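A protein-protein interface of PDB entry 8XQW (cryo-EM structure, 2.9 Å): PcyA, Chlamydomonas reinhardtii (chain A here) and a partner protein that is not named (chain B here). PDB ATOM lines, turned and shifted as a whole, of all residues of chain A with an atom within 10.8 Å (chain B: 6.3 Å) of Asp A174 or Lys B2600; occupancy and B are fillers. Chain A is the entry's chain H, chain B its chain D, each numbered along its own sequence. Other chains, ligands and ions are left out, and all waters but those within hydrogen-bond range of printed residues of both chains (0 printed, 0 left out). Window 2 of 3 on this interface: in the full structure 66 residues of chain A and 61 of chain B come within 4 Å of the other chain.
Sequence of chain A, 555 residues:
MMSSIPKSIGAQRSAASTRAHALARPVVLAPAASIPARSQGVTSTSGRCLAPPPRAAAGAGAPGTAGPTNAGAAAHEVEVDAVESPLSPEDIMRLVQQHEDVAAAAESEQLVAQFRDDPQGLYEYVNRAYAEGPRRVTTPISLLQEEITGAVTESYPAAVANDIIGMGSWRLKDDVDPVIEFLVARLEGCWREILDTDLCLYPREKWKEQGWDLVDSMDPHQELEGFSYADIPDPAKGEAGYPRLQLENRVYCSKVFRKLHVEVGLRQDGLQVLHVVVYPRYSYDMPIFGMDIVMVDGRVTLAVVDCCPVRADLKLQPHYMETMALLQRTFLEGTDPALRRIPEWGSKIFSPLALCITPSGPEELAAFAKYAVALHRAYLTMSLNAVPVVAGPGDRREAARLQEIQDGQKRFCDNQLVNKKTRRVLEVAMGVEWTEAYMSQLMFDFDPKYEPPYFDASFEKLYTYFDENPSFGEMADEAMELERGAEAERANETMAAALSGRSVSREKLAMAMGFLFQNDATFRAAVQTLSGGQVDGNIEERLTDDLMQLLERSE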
ATOM      1  N   GLY A 166      19.469  11.954  21.636  1.00  0.00           N
ATOM      2  CA  GLY A 166      20.157  10.705  21.894  1.00  0.00           C
ATOM      3  C   GLY A 166      21.563  10.716  21.347  1.00  0.00           C
ATOM      4  O   GLY A 166      22.201  11.768  21.311  1.00  0.00           O
ATOM      5  N   MET A 167      22.068   9.563  20.918  1.00  0.00           N
ATOM      6  CA  MET A 167      23.357   9.512  20.238  1.00  0.00           C
ATOM      7  C   MET A 167      23.187  10.062  18.824  1.00  0.00           C
ATOM      8  O   MET A 167      23.203   9.346  17.830  1.00  0.00           O
ATOM      9  CB  MET A 167      23.907   8.095  20.226  1.00  0.00           C
ATOM     10  CG  MET A 167      25.397   8.043  20.392  1.00  0.00           C
ATOM     11  SD  MET A 167      26.062   6.411  20.099  1.00  0.00           S
ATOM     12  CE  MET A 167      27.799   6.787  19.938  1.00  0.00           C
ATOM     13  N   GLY A 168      23.036  11.378  18.766  1.00  0.00           N
ATOM     14  CA  GLY A 168      22.426  12.055  17.645  1.00  0.00           C
ATOM     15  C   GLY A 168      22.890  11.689  16.260  1.00  0.00           C
ATOM     16  O   GLY A 168      22.141  11.077  15.506  1.00  0.00           O
ATOM     17  N   SER A 169      24.113  12.049  15.905  1.00  0.00           N
ATOM     18  CA  SER A 169      24.558  11.902  14.532  1.00  0.00           C
ATOM     19  C   SER A 169      25.939  11.294  14.481  1.00  0.00           C
ATOM     20  O   SER A 169      26.679  11.492  13.518  1.00  0.00           O
ATOM     21  CB  SER A 169      24.556  13.239  13.808  1.00  0.00           C
ATOM     22  OG  SER A 169      23.243  13.631  13.488  1.00  0.00           O
ATOM     23  N   TRP A 170      26.322  10.567  15.519  1.00  0.00           N
ATOM     24  CA  TRP A 170      27.577   9.844  15.469  1.00  0.00           C
ATOM     25  C   TRP A 170      27.551   8.903  14.283  1.00  0.00           C
ATOM     26  O   TRP A 170      26.542   8.251  14.021  1.00  0.00           O
ATOM     27  CB  TRP A 170      27.793   9.065  16.754  1.00  0.00           C
ATOM     28  CG  TRP A 170      28.071   9.911  17.915  1.00  0.00           C
ATOM     29  CD1 TRP A 170      27.199  10.709  18.564  1.00  0.00           C
ATOM     30  CD2 TRP A 170      29.313  10.034  18.593  1.00  0.00           C
ATOM     31  NE1 TRP A 170      27.820  11.335  19.607  1.00  0.00           N
ATOM     32  CE2 TRP A 170      29.125  10.931  19.643  1.00  0.00           C
ATOM     33  CE3 TRP A 170      30.572   9.468  18.414  1.00  0.00           C
ATOM     34  CZ2 TRP A 170      30.142  11.279  20.505  1.00  0.00           C
ATOM     35  CZ3 TRP A 170      31.574   9.816  19.269  1.00  0.00           C
ATOM     36  CH2 TRP A 170      31.358  10.708  20.298  1.00  0.00           C
ATOM     37  N   ARG A 171      28.652   8.848  13.544  1.00  0.00           N
ATOM     38  CA  ARG A 171      28.649   8.039  12.337  1.00  0.00           C
ATOM     39  C   ARG A 171      28.848   6.567  12.630  1.00  0.00           C
ATOM     40  O   ARG A 171      28.583   5.738  11.760  1.00  0.00           O
ATOM     41  CB  ARG A 171      29.717   8.530  11.376  1.00  0.00           C
ATOM     42  CG  ARG A 171      29.249   9.685  10.552  1.00  0.00           C
ATOM     43  CD  ARG A 171      30.397  10.548  10.152  1.00  0.00           C
ATOM     44  NE  ARG A 171      31.150  10.989  11.310  1.00  0.00           N
ATOM     45  CZ  ARG A 171      32.180  11.819  11.252  1.00  0.00           C
ATOM     46  NH1 ARG A 171      32.581  12.304  10.092  1.00  0.00           N
ATOM     47  NH2 ARG A 171      32.809  12.160  12.361  1.00  0.00           N
ATOM     48  N   LEU A 172      29.294   6.220  13.831  1.00  0.00           N
ATOM     49  CA  LEU A 172      29.543   4.835  14.187  1.00  0.00           C
ATOM     50  C   LEU A 172      28.463   4.257  15.077  1.00  0.00           C
ATOM     51  O   LEU A 172      28.635   3.159  15.603  1.00  0.00           O
ATOM     52  CB  LEU A 172      30.898   4.693  14.864  1.00  0.00           C
ATOM     53  CG  LEU A 172      32.080   4.509  13.929  1.00  0.00           C
ATOM     54  CD1 LEU A 172      33.167   3.808  14.670  1.00  0.00           C
ATOM     55  CD2 LEU A 172      31.668   3.718  12.726  1.00  0.00           C
ATOM     56  N   LYS A 173      27.351   4.957  15.258  1.00  0.00           N
ATOM     57  CA  LYS A 173      26.222   4.307  15.890  1.00  0.00           C
ATOM     58  C   LYS A 173      25.759   3.162  14.999  1.00  0.00           C
ATOM     59  O   LYS A 173      26.272   2.961  13.899  1.00  0.00           O
ATOM     60  CB  LYS A 173      25.102   5.301  16.159  1.00  0.00           C
ATOM     61  CG  LYS A 173      24.455   5.881  14.932  1.00  0.00           C
ATOM     62  CD  LYS A 173      23.332   6.817  15.331  1.00  0.00           C
ATOM     63  CE  LYS A 173      22.592   7.358  14.133  1.00  0.00           C
ATOM     64  NZ  LYS A 173      23.490   7.676  13.003  1.00  0.00           N
ATOM     65  N   ASP A 174      24.788   2.399  15.499  1.00  0.00           N
ATOM     66  CA  ASP A 174      24.319   1.152  14.896  1.00  0.00           C
ATOM     67  C   ASP A 174      25.314   0.031  15.159  1.00  0.00           C
ATOM     68  O   ASP A 174      25.025  -1.134  14.890  1.00  0.00           O
ATOM     69  CB  ASP A 174      24.098   1.295  13.388  1.00  0.00           C
ATOM     70  CG  ASP A 174      22.907   2.159  13.051  1.00  0.00           C
ATOM     71  OD1 ASP A 174      22.087   2.412  13.952  1.00  0.00           O
ATOM     72  OD2 ASP A 174      22.805   2.610  11.891  1.00  0.00           O
ATOM     73  N   ASP A 175      26.483   0.367  15.695  1.00  0.00           N
ATOM     74  CA  ASP A 175      27.496  -0.615  16.051  1.00  0.00           C
ATOM     75  C   ASP A 175      27.819  -0.604  17.529  1.00  0.00           C
ATOM     76  O   ASP A 175      28.640  -1.403  17.979  1.00  0.00           O
ATOM     77  CB  ASP A 175      28.784  -0.364  15.268  1.00  0.00           C
ATOM     78  CG  ASP A 175      28.558  -0.305  13.787  1.00  0.00           C
ATOM     79  OD1 ASP A 175      27.535  -0.842  13.323  1.00  0.00           O
ATOM     80  OD2 ASP A 175      29.405   0.279  13.081  1.00  0.00           O
ATOM     81  N   VAL A 176      27.195   0.274  18.289  1.00  0.00           N
ATOM     82  CA  VAL A 176      27.575   0.556  19.660  1.00  0.00           C
ATOM     83  C   VAL A 176      26.612  -0.151  20.599  1.00  0.00           C
ATOM     84  O   VAL A 176      25.395  -0.137  20.397  1.00  0.00           O
ATOM     85  CB  VAL A 176      27.580   2.081  19.883  1.00  0.00           C
ATOM     86  CG1 VAL A 176      27.614   2.402  21.333  1.00  0.00           C
ATOM     87  CG2 VAL A 176      28.759   2.703  19.189  1.00  0.00           C
ATOM     88  N   ASP A 177      27.165  -0.793  21.622  1.00  0.00           N
ATOM     89  CA  ASP A 177      26.341  -1.459  22.612  1.00  0.00           C
ATOM     90  C   ASP A 177      25.425  -0.453  23.300  1.00  0.00           C
ATOM     91  O   ASP A 177      25.803   0.698  23.499  1.00  0.00           O
ATOM     92  CB  ASP A 177      27.217  -2.146  23.646  1.00  0.00           C
ATOM     93  CG  ASP A 177      26.418  -2.859  24.705  1.00  0.00           C
ATOM     94  OD1 ASP A 177      25.968  -3.994  24.449  1.00  0.00           O
ATOM     95  OD2 ASP A 177      26.230  -2.285  25.794  1.00  0.00           O
ATOM     96  N   PRO A 178      24.210  -0.863  23.668  1.00  0.00           N
ATOM     97  CA  PRO A 178      23.260   0.101  24.242  1.00  0.00           C
ATOM     98  C   PRO A 178      23.740   0.804  25.497  1.00  0.00           C
ATOM     99  O   PRO A 178      23.313   1.937  25.749  1.00  0.00           O
ATOM    100  CB  PRO A 178      22.031  -0.767  24.523  1.00  0.00           C
ATOM    101  CG  PRO A 178      22.101  -1.822  23.515  1.00  0.00           C
ATOM    102  CD  PRO A 178      23.551  -2.122  23.303  1.00  0.00           C
ATOM    103  N   ILE A 180      26.883   1.850  26.167  1.00  0.00           N
ATOM    104  CA  ILE A 180      27.725   2.948  25.721  1.00  0.00           C
ATOM    105  C   ILE A 180      26.883   4.031  25.072  1.00  0.00           C
ATOM    106  O   ILE A 180      27.157   5.225  25.228  1.00  0.00           O
ATOM    107  CB  ILE A 180      28.809   2.416  24.776  1.00  0.00           C
ATOM    108  CG1 ILE A 180      29.773   1.528  25.548  1.00  0.00           C
ATOM    109  CG2 ILE A 180      29.554   3.542  24.133  1.00  0.00           C
ATOM    110  CD1 ILE A 180      31.000   1.185  24.782  1.00  0.00           C
ATOM    111  N   GLU A 181      25.831   3.641  24.355  1.00  0.00           N
ATOM    112  CA  GLU A 181      24.912   4.621  23.796  1.00  0.00           C
ATOM    113  C   GLU A 181      24.300   5.479  24.890  1.00  0.00           C
ATOM    114  O   GLU A 181      24.291   6.712  24.798  1.00  0.00           O
ATOM    115  CB  GLU A 181      23.811   3.918  23.015  1.00  0.00           C
ATOM    116  CG  GLU A 181      24.090   3.733  21.550  1.00  0.00           C
ATOM    117  CD  GLU A 181      22.814   3.537  20.752  1.00  0.00           C
ATOM    118  OE1 GLU A 181      22.698   2.516  20.039  1.00  0.00           O
ATOM    119  OE2 GLU A 181      21.926   4.410  20.830  1.00  0.00           O
ATOM    120  N   PHE A 182      23.780   4.840  25.936  1.00  0.00           N
ATOM    121  CA  PHE A 182      23.159   5.579  27.028  1.00  0.00           C
ATOM    122  C   PHE A 182      24.145   6.542  27.668  1.00  0.00           C
ATOM    123  O   PHE A 182      23.833   7.719  27.888  1.00  0.00           O
ATOM    124  CB  PHE A 182      22.613   4.591  28.054  1.00  0.00           C
ATOM    125  CG  PHE A 182      22.280   5.197  29.370  1.00  0.00           C
ATOM    126  CD1 PHE A 182      21.031   5.710  29.610  1.00  0.00           C
ATOM    127  CD2 PHE A 182      23.201   5.218  30.383  1.00  0.00           C
ATOM    128  CE1 PHE A 182      20.724   6.253  30.819  1.00  0.00           C
ATOM    129  CE2 PHE A 182      22.897   5.765  31.590  1.00  0.00           C
ATOM    130  CZ  PHE A 182      21.659   6.279  31.810  1.00  0.00           C
ATOM    131  N   TYR A 229      34.059   3.186   6.782  1.00  0.00           N
ATOM    132  CA  TYR A 229      33.176   2.400   7.626  1.00  0.00           C
ATOM    133  C   TYR A 229      32.022   1.803   6.846  1.00  0.00           C
ATOM    134  O   TYR A 229      31.284   0.985   7.396  1.00  0.00           O
ATOM    135  CB  TYR A 229      32.641   3.250   8.774  1.00  0.00           C
ATOM    136  CG  TYR A 229      31.667   4.301   8.334  1.00  0.00           C
ATOM    137  CD1 TYR A 229      32.107   5.485   7.794  1.00  0.00           C
ATOM    138  CD2 TYR A 229      30.311   4.105   8.451  1.00  0.00           C
ATOM    139  CE1 TYR A 229      31.229   6.435   7.383  1.00  0.00           C
ATOM    140  CE2 TYR A 229      29.426   5.051   8.043  1.00  0.00           C
ATOM    141  CZ  TYR A 229      29.889   6.211   7.508  1.00  0.00           C
ATOM    142  OH  TYR A 229      28.998   7.162   7.098  1.00  0.00           O
ATOM    143  N   ALA A 230      31.851   2.191   5.585  1.00  0.00           N
ATOM    144  CA  ALA A 230      30.750   1.707   4.772  1.00  0.00           C
ATOM    145  C   ALA A 230      31.178   1.051   3.477  1.00  0.00           C
ATOM    146  O   ALA A 230      30.432   0.214   2.965  1.00  0.00           O
ATOM    147  CB  ALA A 230      29.789   2.850   4.434  1.00  0.00           C
ATOM    148  N   ASP A 234      33.976  -6.286   6.469  1.00  0.00           N
ATOM    149  CA  ASP A 234      34.820  -6.738   7.558  1.00  0.00           C
ATOM    150  C   ASP A 234      35.689  -7.906   7.105  1.00  0.00           C
ATOM    151  O   ASP A 234      35.188  -8.850   6.492  1.00  0.00           O
ATOM    152  CB  ASP A 234      33.973  -7.160   8.752  1.00  0.00           C
ATOM    153  CG  ASP A 234      33.546  -5.988   9.600  1.00  0.00           C
ATOM    154  OD1 ASP A 234      34.007  -4.860   9.332  1.00  0.00           O
ATOM    155  OD2 ASP A 234      32.748  -6.190  10.538  1.00  0.00           O
ATOM    156  N   GLN A 246      38.116   0.655  14.801  1.00  0.00           N
ATOM    157  CA  GLN A 246      37.478   1.909  14.434  1.00  0.00           C
ATOM    158  C   GLN A 246      37.417   2.826  15.639  1.00  0.00           C
ATOM    159  O   GLN A 246      37.111   2.385  16.743  1.00  0.00           O
ATOM    160  CB  GLN A 246      36.076   1.687  13.918  1.00  0.00           C
ATOM    161  CG  GLN A 246      35.944   0.515  13.017  1.00  0.00           C
ATOM    162  CD  GLN A 246      34.976   0.779  11.917  1.00  0.00           C
ATOM    163  OE1 GLN A 246      33.830   0.352  11.968  1.00  0.00           O
ATOM    164  NE2 GLN A 246      35.425   1.497  10.908  1.00  0.00           N
ATOM    165  N   GLU A 248      36.134   6.928  16.932  1.00  0.00           N
ATOM    166  CA  GLU A 248      35.481   8.191  16.644  1.00  0.00           C
ATOM    167  C   GLU A 248      35.614   9.112  17.842  1.00  0.00           C
ATOM    168  O   GLU A 248      35.350   8.705  18.974  1.00  0.00           O
ATOM    169  CB  GLU A 248      34.013   7.990  16.294  1.00  0.00           C
ATOM    170  CG  GLU A 248      33.245   9.282  16.225  1.00  0.00           C
ATOM    171  CD  GLU A 248      32.190   9.297  15.149  1.00  0.00           C
ATOM    172  OE1 GLU A 248      31.652   8.221  14.838  1.00  0.00           O
ATOM    173  OE2 GLU A 248      31.893  10.388  14.619  1.00  0.00           O
ATOM    174  N   VAL A 264      35.101   6.952  21.315  1.00  0.00           N
ATOM    175  CA  VAL A 264      34.592   5.589  21.315  1.00  0.00           C
ATOM    176  C   VAL A 264      35.446   4.758  20.375  1.00  0.00           C
ATOM    177  O   VAL A 264      35.892   5.253  19.336  1.00  0.00           O
ATOM    178  CB  VAL A 264      33.116   5.530  20.891  1.00  0.00           C
ATOM    179  CG1 VAL A 264      32.571   4.155  21.110  1.00  0.00           C
ATOM    180  CG2 VAL A 264      32.314   6.513  21.680  1.00  0.00           C
ATOM    181  N   LEU A 266      35.860   0.644  18.647  1.00  0.00           N
ATOM    182  CA  LEU A 266      35.335  -0.688  18.398  1.00  0.00           C
ATOM    183  C   LEU A 266      36.413  -1.545  17.771  1.00  0.00           C
ATOM    184  O   LEU A 266      37.231  -1.051  16.991  1.00  0.00           O
ATOM    185  CB  LEU A 266      34.138  -0.667  17.466  1.00  0.00           C
ATOM    186  CG  LEU A 266      32.969   0.218  17.853  1.00  0.00           C
ATOM    187  CD1 LEU A 266      32.430   0.898  16.637  1.00  0.00           C
ATOM    188  CD2 LEU A 266      31.906  -0.624  18.465  1.00  0.00           C
ATOM    189  N   GLN A 272      34.759  -3.141  23.034  1.00  0.00           N
ATOM    190  CA  GLN A 272      34.306  -1.765  22.894  1.00  0.00           C
ATOM    191  C   GLN A 272      34.745  -0.966  24.103  1.00  0.00           C
ATOM    192  O   GLN A 272      34.489  -1.368  25.240  1.00  0.00           O
ATOM    193  CB  GLN A 272      32.789  -1.689  22.757  1.00  0.00           C
ATOM    194  CG  GLN A 272      32.268  -2.314  21.506  1.00  0.00           C
ATOM    195  CD  GLN A 272      30.777  -2.276  21.426  1.00  0.00           C
ATOM    196  OE1 GLN A 272      30.104  -1.905  22.378  1.00  0.00           O
ATOM    197  NE2 GLN A 272      30.239  -2.675  20.289  1.00  0.00           N
ATOM    198  N   SER B2595      19.354   8.963  11.469  1.00  0.00           N
ATOM    199  CA  SER B2595      18.344   7.975  11.799  1.00  0.00           C
ATOM    200  C   SER B2595      18.981   6.687  12.285  1.00  0.00           C
ATOM    201  O   SER B2595      20.041   6.284  11.808  1.00  0.00           O
ATOM    202  CB  SER B2595      17.471   7.689  10.586  1.00  0.00           C
ATOM    203  OG  SER B2595      16.647   8.798  10.293  1.00  0.00           O
ATOM    204  N   LYS B2596      18.313   6.038  13.226  1.00  0.00           N
ATOM    205  CA  LYS B2596      18.754   4.769  13.776  1.00  0.00           C
ATOM    206  C   LYS B2596      18.282   3.630  12.885  1.00  0.00           C
ATOM    207  O   LYS B2596      17.096   3.544  12.562  1.00  0.00           O
ATOM    208  CB  LYS B2596      18.198   4.595  15.187  1.00  0.00           C
ATOM    209  CG  LYS B2596      19.012   3.704  16.081  1.00  0.00           C
ATOM    210  CD  LYS B2596      20.470   4.049  15.983  1.00  0.00           C
ATOM    211  CE  LYS B2596      21.238   3.556  17.191  1.00  0.00           C
ATOM    212  NZ  LYS B2596      21.403   4.631  18.204  1.00  0.00           N
ATOM    213  N   ASN B2597      19.205   2.762  12.491  1.00  0.00           N
ATOM    214  CA  ASN B2597      18.870   1.568  11.724  1.00  0.00           C
ATOM    215  C   ASN B2597      18.377   0.495  12.682  1.00  0.00           C
ATOM    216  O   ASN B2597      19.161  -0.055  13.459  1.00  0.00           O
ATOM    217  CB  ASN B2597      20.090   1.097  10.947  1.00  0.00           C
ATOM    218  CG  ASN B2597      19.799  -0.080  10.074  1.00  0.00           C
ATOM    219  OD1 ASN B2597      18.650  -0.375   9.780  1.00  0.00           O
ATOM    220  ND2 ASN B2597      20.843  -0.763   9.645  1.00  0.00           N
ATOM    221  N   LEU B2598      17.085   0.191  12.634  1.00  0.00           N
ATOM    222  CA  LEU B2598      16.471  -0.694  13.615  1.00  0.00           C
ATOM    223  C   LEU B2598      16.690  -2.170  13.339  1.00  0.00           C
ATOM    224  O   LEU B2598      16.344  -2.995  14.190  1.00  0.00           O
ATOM    225  CB  LEU B2598      14.974  -0.443  13.681  1.00  0.00           C
ATOM    226  CG  LEU B2598      14.555   0.912  14.208  1.00  0.00           C
ATOM    227  CD1 LEU B2598      13.087   0.876  14.474  1.00  0.00           C
ATOM    228  CD2 LEU B2598      15.307   1.216  15.472  1.00  0.00           C
ATOM    229  N   VAL B2599      17.214  -2.532  12.173  1.00  0.00           N
ATOM    230  CA  VAL B2599      17.403  -3.941  11.858  1.00  0.00           C
ATOM    231  C   VAL B2599      18.304  -4.596  12.888  1.00  0.00           C
ATOM    232  O   VAL B2599      18.072  -5.737  13.303  1.00  0.00           O
ATOM    233  CB  VAL B2599      17.971  -4.087  10.440  1.00  0.00           C
ATOM    234  CG1 VAL B2599      18.574  -5.445  10.259  1.00  0.00           C
ATOM    235  CG2 VAL B2599      16.882  -3.859   9.438  1.00  0.00           C
ATOM    236  N   LYS B2600      19.333  -3.877  13.327  1.00  0.00           N
ATOM    237  CA  LYS B2600      20.287  -4.421  14.284  1.00  0.00           C
ATOM    238  C   LYS B2600      19.583  -4.934  15.530  1.00  0.00           C
ATOM    239  O   LYS B2600      19.695  -6.111  15.883  1.00  0.00           O
ATOM    240  CB  LYS B2600      21.307  -3.348  14.642  1.00  0.00           C
ATOM    241  CG  LYS B2600      22.044  -2.786  13.445  1.00  0.00           C
ATOM    242  CD  LYS B2600      23.138  -3.734  13.007  1.00  0.00           C
ATOM    243  CE  LYS B2600      24.084  -4.020  14.160  1.00  0.00           C
ATOM    244  NZ  LYS B2600      24.244  -5.471  14.417  1.00  0.00           N
ATOM    245  N   SER B2601      18.819  -4.069  16.192  1.00  0.00           N
ATOM    246  CA  SER B2601      18.139  -4.470  17.413  1.00  0.00           C
ATOM    247  C   SER B2601      16.963  -5.397  17.161  1.00  0.00           C
ATOM    248  O   SER B2601      16.650  -6.218  18.026  1.00  0.00           O
ATOM    249  CB  SER B2601      17.675  -3.236  18.171  1.00  0.00           C
ATOM    250  OG  SER B2601      17.367  -2.193  17.272  1.00  0.00           O
ATOM    251  N   LEU B2602      16.299  -5.296  16.012  1.00  0.00           N
ATOM    252  CA  LEU B2602      15.172  -6.187  15.763  1.00  0.00           C
ATOM    253  C   LEU B2602      15.634  -7.613  15.502  1.00  0.00           C
ATOM    254  O   LEU B2602      14.883  -8.560  15.745  1.00  0.00           O
ATOM    255  CB  LEU B2602      14.340  -5.682  14.592  1.00  0.00           C
ATOM    256  CG  LEU B2602      13.302  -4.629  14.941  1.00  0.00           C
ATOM    257  CD1 LEU B2602      12.681  -4.074  13.687  1.00  0.00           C
ATOM    258  CD2 LEU B2602      12.251  -5.229  15.830  1.00  0.00           C
ATOM    259  N   LYS B2603      16.854  -7.788  15.000  1.00  0.00           N
ATOM    260  CA  LYS B2603      17.388  -9.126  14.786  1.00  0.00           C
ATOM    261  C   LYS B2603      18.296  -9.601  15.909  1.00  0.00           C
ATOM    262  O   LYS B2603      18.589 -10.798  15.978  1.00  0.00           O
ATOM    263  CB  LYS B2603      18.158  -9.192  13.464  1.00  0.00           C
ATOM    264  CG  LYS B2603      17.285  -9.073  12.234  1.00  0.00           C
ATOM    265  CD  LYS B2603      17.523 -10.214  11.263  1.00  0.00           C
ATOM    266  CE  LYS B2603      16.767 -11.455  11.691  1.00  0.00           C
ATOM    267  NZ  LYS B2603      17.234 -12.666  10.969  1.00  0.00           N
ATOM    268  N   GLN B2604      18.747  -8.706  16.785  1.00  0.00           N
ATOM    269  CA  GLN B2604      19.602  -9.114  17.892  1.00  0.00           C
ATOM    270  C   GLN B2604      18.795  -9.541  19.110  1.00  0.00           C
ATOM    271  O   GLN B2604      18.985 -10.646  19.628  1.00  0.00           O
ATOM    272  CB  GLN B2604      20.554  -7.976  18.269  1.00  0.00           C
ATOM    273  CG  GLN B2604      21.192  -8.128  19.631  1.00  0.00           C
ATOM    274  CD  GLN B2604      22.190  -9.266  19.676  1.00  0.00           C
ATOM    275  OE1 GLN B2604      23.036  -9.399  18.793  1.00  0.00           O
ATOM    276  NE2 GLN B2604      22.096 -10.097  20.711  1.00  0.00           N
ATOM    277  N   ALA B2605      17.879  -8.684  19.567  1.00  0.00           N
ATOM    278  CA  ALA B2605      17.096  -8.981  20.760  1.00  0.00           C
ATOM    279  C   ALA B2605      16.251 -10.240  20.608  1.00  0.00           C
ATOM    280  O   ALA B2605      15.597 -10.654  21.570  1.00  0.00           O
ATOM    281  CB  ALA B2605      16.206  -7.789  21.113  1.00  0.00           C
ATOM    282  N   PRO B2633      26.398 -11.258  12.707  1.00  0.00           N
ATOM    283  CA  PRO B2633      25.389 -10.201  12.772  1.00  0.00           C
ATOM    284  C   PRO B2633      25.620  -8.791  12.218  1.00  0.00           C
ATOM    285  O   PRO B2633      24.644  -8.028  12.190  1.00  0.00           O
ATOM    286  CB  PRO B2633      25.221 -10.138  14.292  1.00  0.00           C
ATOM    287  CG  PRO B2633      25.278 -11.578  14.716  1.00  0.00           C
ATOM    288  CD  PRO B2633      26.409 -12.123  13.871  1.00  0.00           C
ATOM    289  N   LYS B2634      26.840  -8.431  11.828  1.00  0.00           N
ATOM    290  CA  LYS B2634      27.059  -7.101  11.212  1.00  0.00           C
ATOM    291  C   LYS B2634      26.906  -7.236   9.702  1.00  0.00           C
ATOM    292  O   LYS B2634      26.227  -6.405   9.080  1.00  0.00           O
ATOM    293  CB  LYS B2634      28.467  -6.557  11.466  1.00  0.00           C
ATOM    294  CG  LYS B2634      28.562  -5.043  11.547  1.00  0.00           C
ATOM    295  CD  LYS B2634      29.559  -4.451  10.560  1.00  0.00           C
ATOM    296  CE  LYS B2634      30.389  -3.368  11.175  1.00  0.00           C
ATOM    297  NZ  LYS B2634      31.657  -3.167  10.467  1.00  0.00           N
ATOM    298  N   SER B2637      23.230  -7.336   8.455  1.00  0.00           N
ATOM    299  CA  SER B2637      22.367  -6.168   8.416  1.00  0.00           C
ATOM    300  C   SER B2637      22.401  -5.421   7.090  1.00  0.00           C
ATOM    301  O   SER B2637      21.818  -4.338   7.002  1.00  0.00           O
ATOM    302  CB  SER B2637      22.753  -5.213   9.536  1.00  0.00           C
ATOM    303  OG  SER B2637      23.905  -4.480   9.174  1.00  0.00           O
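Of chain B, only Lys B2596, Asn B2597 and Lys B2600 come within 4 Å of Asp A174. Printed residues of chain A within 4 Å of Lys B2600: Asp A174. Of chain A, only Asp A174 comes within 4 Å of Asn B2597. No residue of chain A comes within 4 Å of Val B2599. Gln B2604 touches none of the printed residues of chain A. No residue of chain A comes within 4 Å of Ser B2637. Of the printed residues of chain A, Ser B2595 touches Lys A173 (3.6 Å). Of the printed residues of chain A, Lys B2634 touches Asp A234. Of the printed residues of chain B, Glu A181 touches Lys B2596 (2.7 Å). Of the printed residues of chain B, Lys A173 touches Ser B2595. Printed residues of chain B within 4 Å of Asp A234: Lys B2634 (3.1 Å). The nearest residue of chain B that does not touch Asp A174 is Ser B2595 (4.6 Å). The nearest residue of chain A that does not touch Lys B2600 is Asp A175 (4.8 Å).
The side-chain amino group (NZ) of Lys B2596 lies within salt-bridge range of the side-chain carboxylate (OE2) of Glu A181 (2.7 Å). OD1 of Asp A174 is in hydrogen-bond range of N of Asn B2597. NZ of Lys B2634 is in salt-bridge range of OD1 of Asp A234 (3.1 Å).
Of the 24 printed residues of chain A, 4 touch a printed residue of chain B. Printed residues of chain A that touch a printed residue of chain B: Lys A173, Asp A174, Glu A181 and Asp A234. Of the 14 printed residues of chain B, 5 touch a printed residue of chain A. Among the printed residues, 6 pairs touch across the chains.
The backbone carbonyl oxygen (O) of Trp A170 lies within hydrogen-bond range of the side-chain amino group (NZ) of Lys A173 (3.3 Å). NZ of Lys B2600 is in hydrogen-bond range of O of Pro B2633 (3.4 Å). The side-chain hydroxyl (OG) of Ser B2637 sits at hydrogen-bond distance from the backbone carbonyl oxygen (O) of Lys B2634, at 3.0 Å.
Among the printed residues, pairs that only touch across the chains: Asp A174 with Lys B2596 (3.1 Å), Asp A174 with Lys B2600 (3.1 Å) and Lys A173 with Ser B2595 (3.6 Å).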
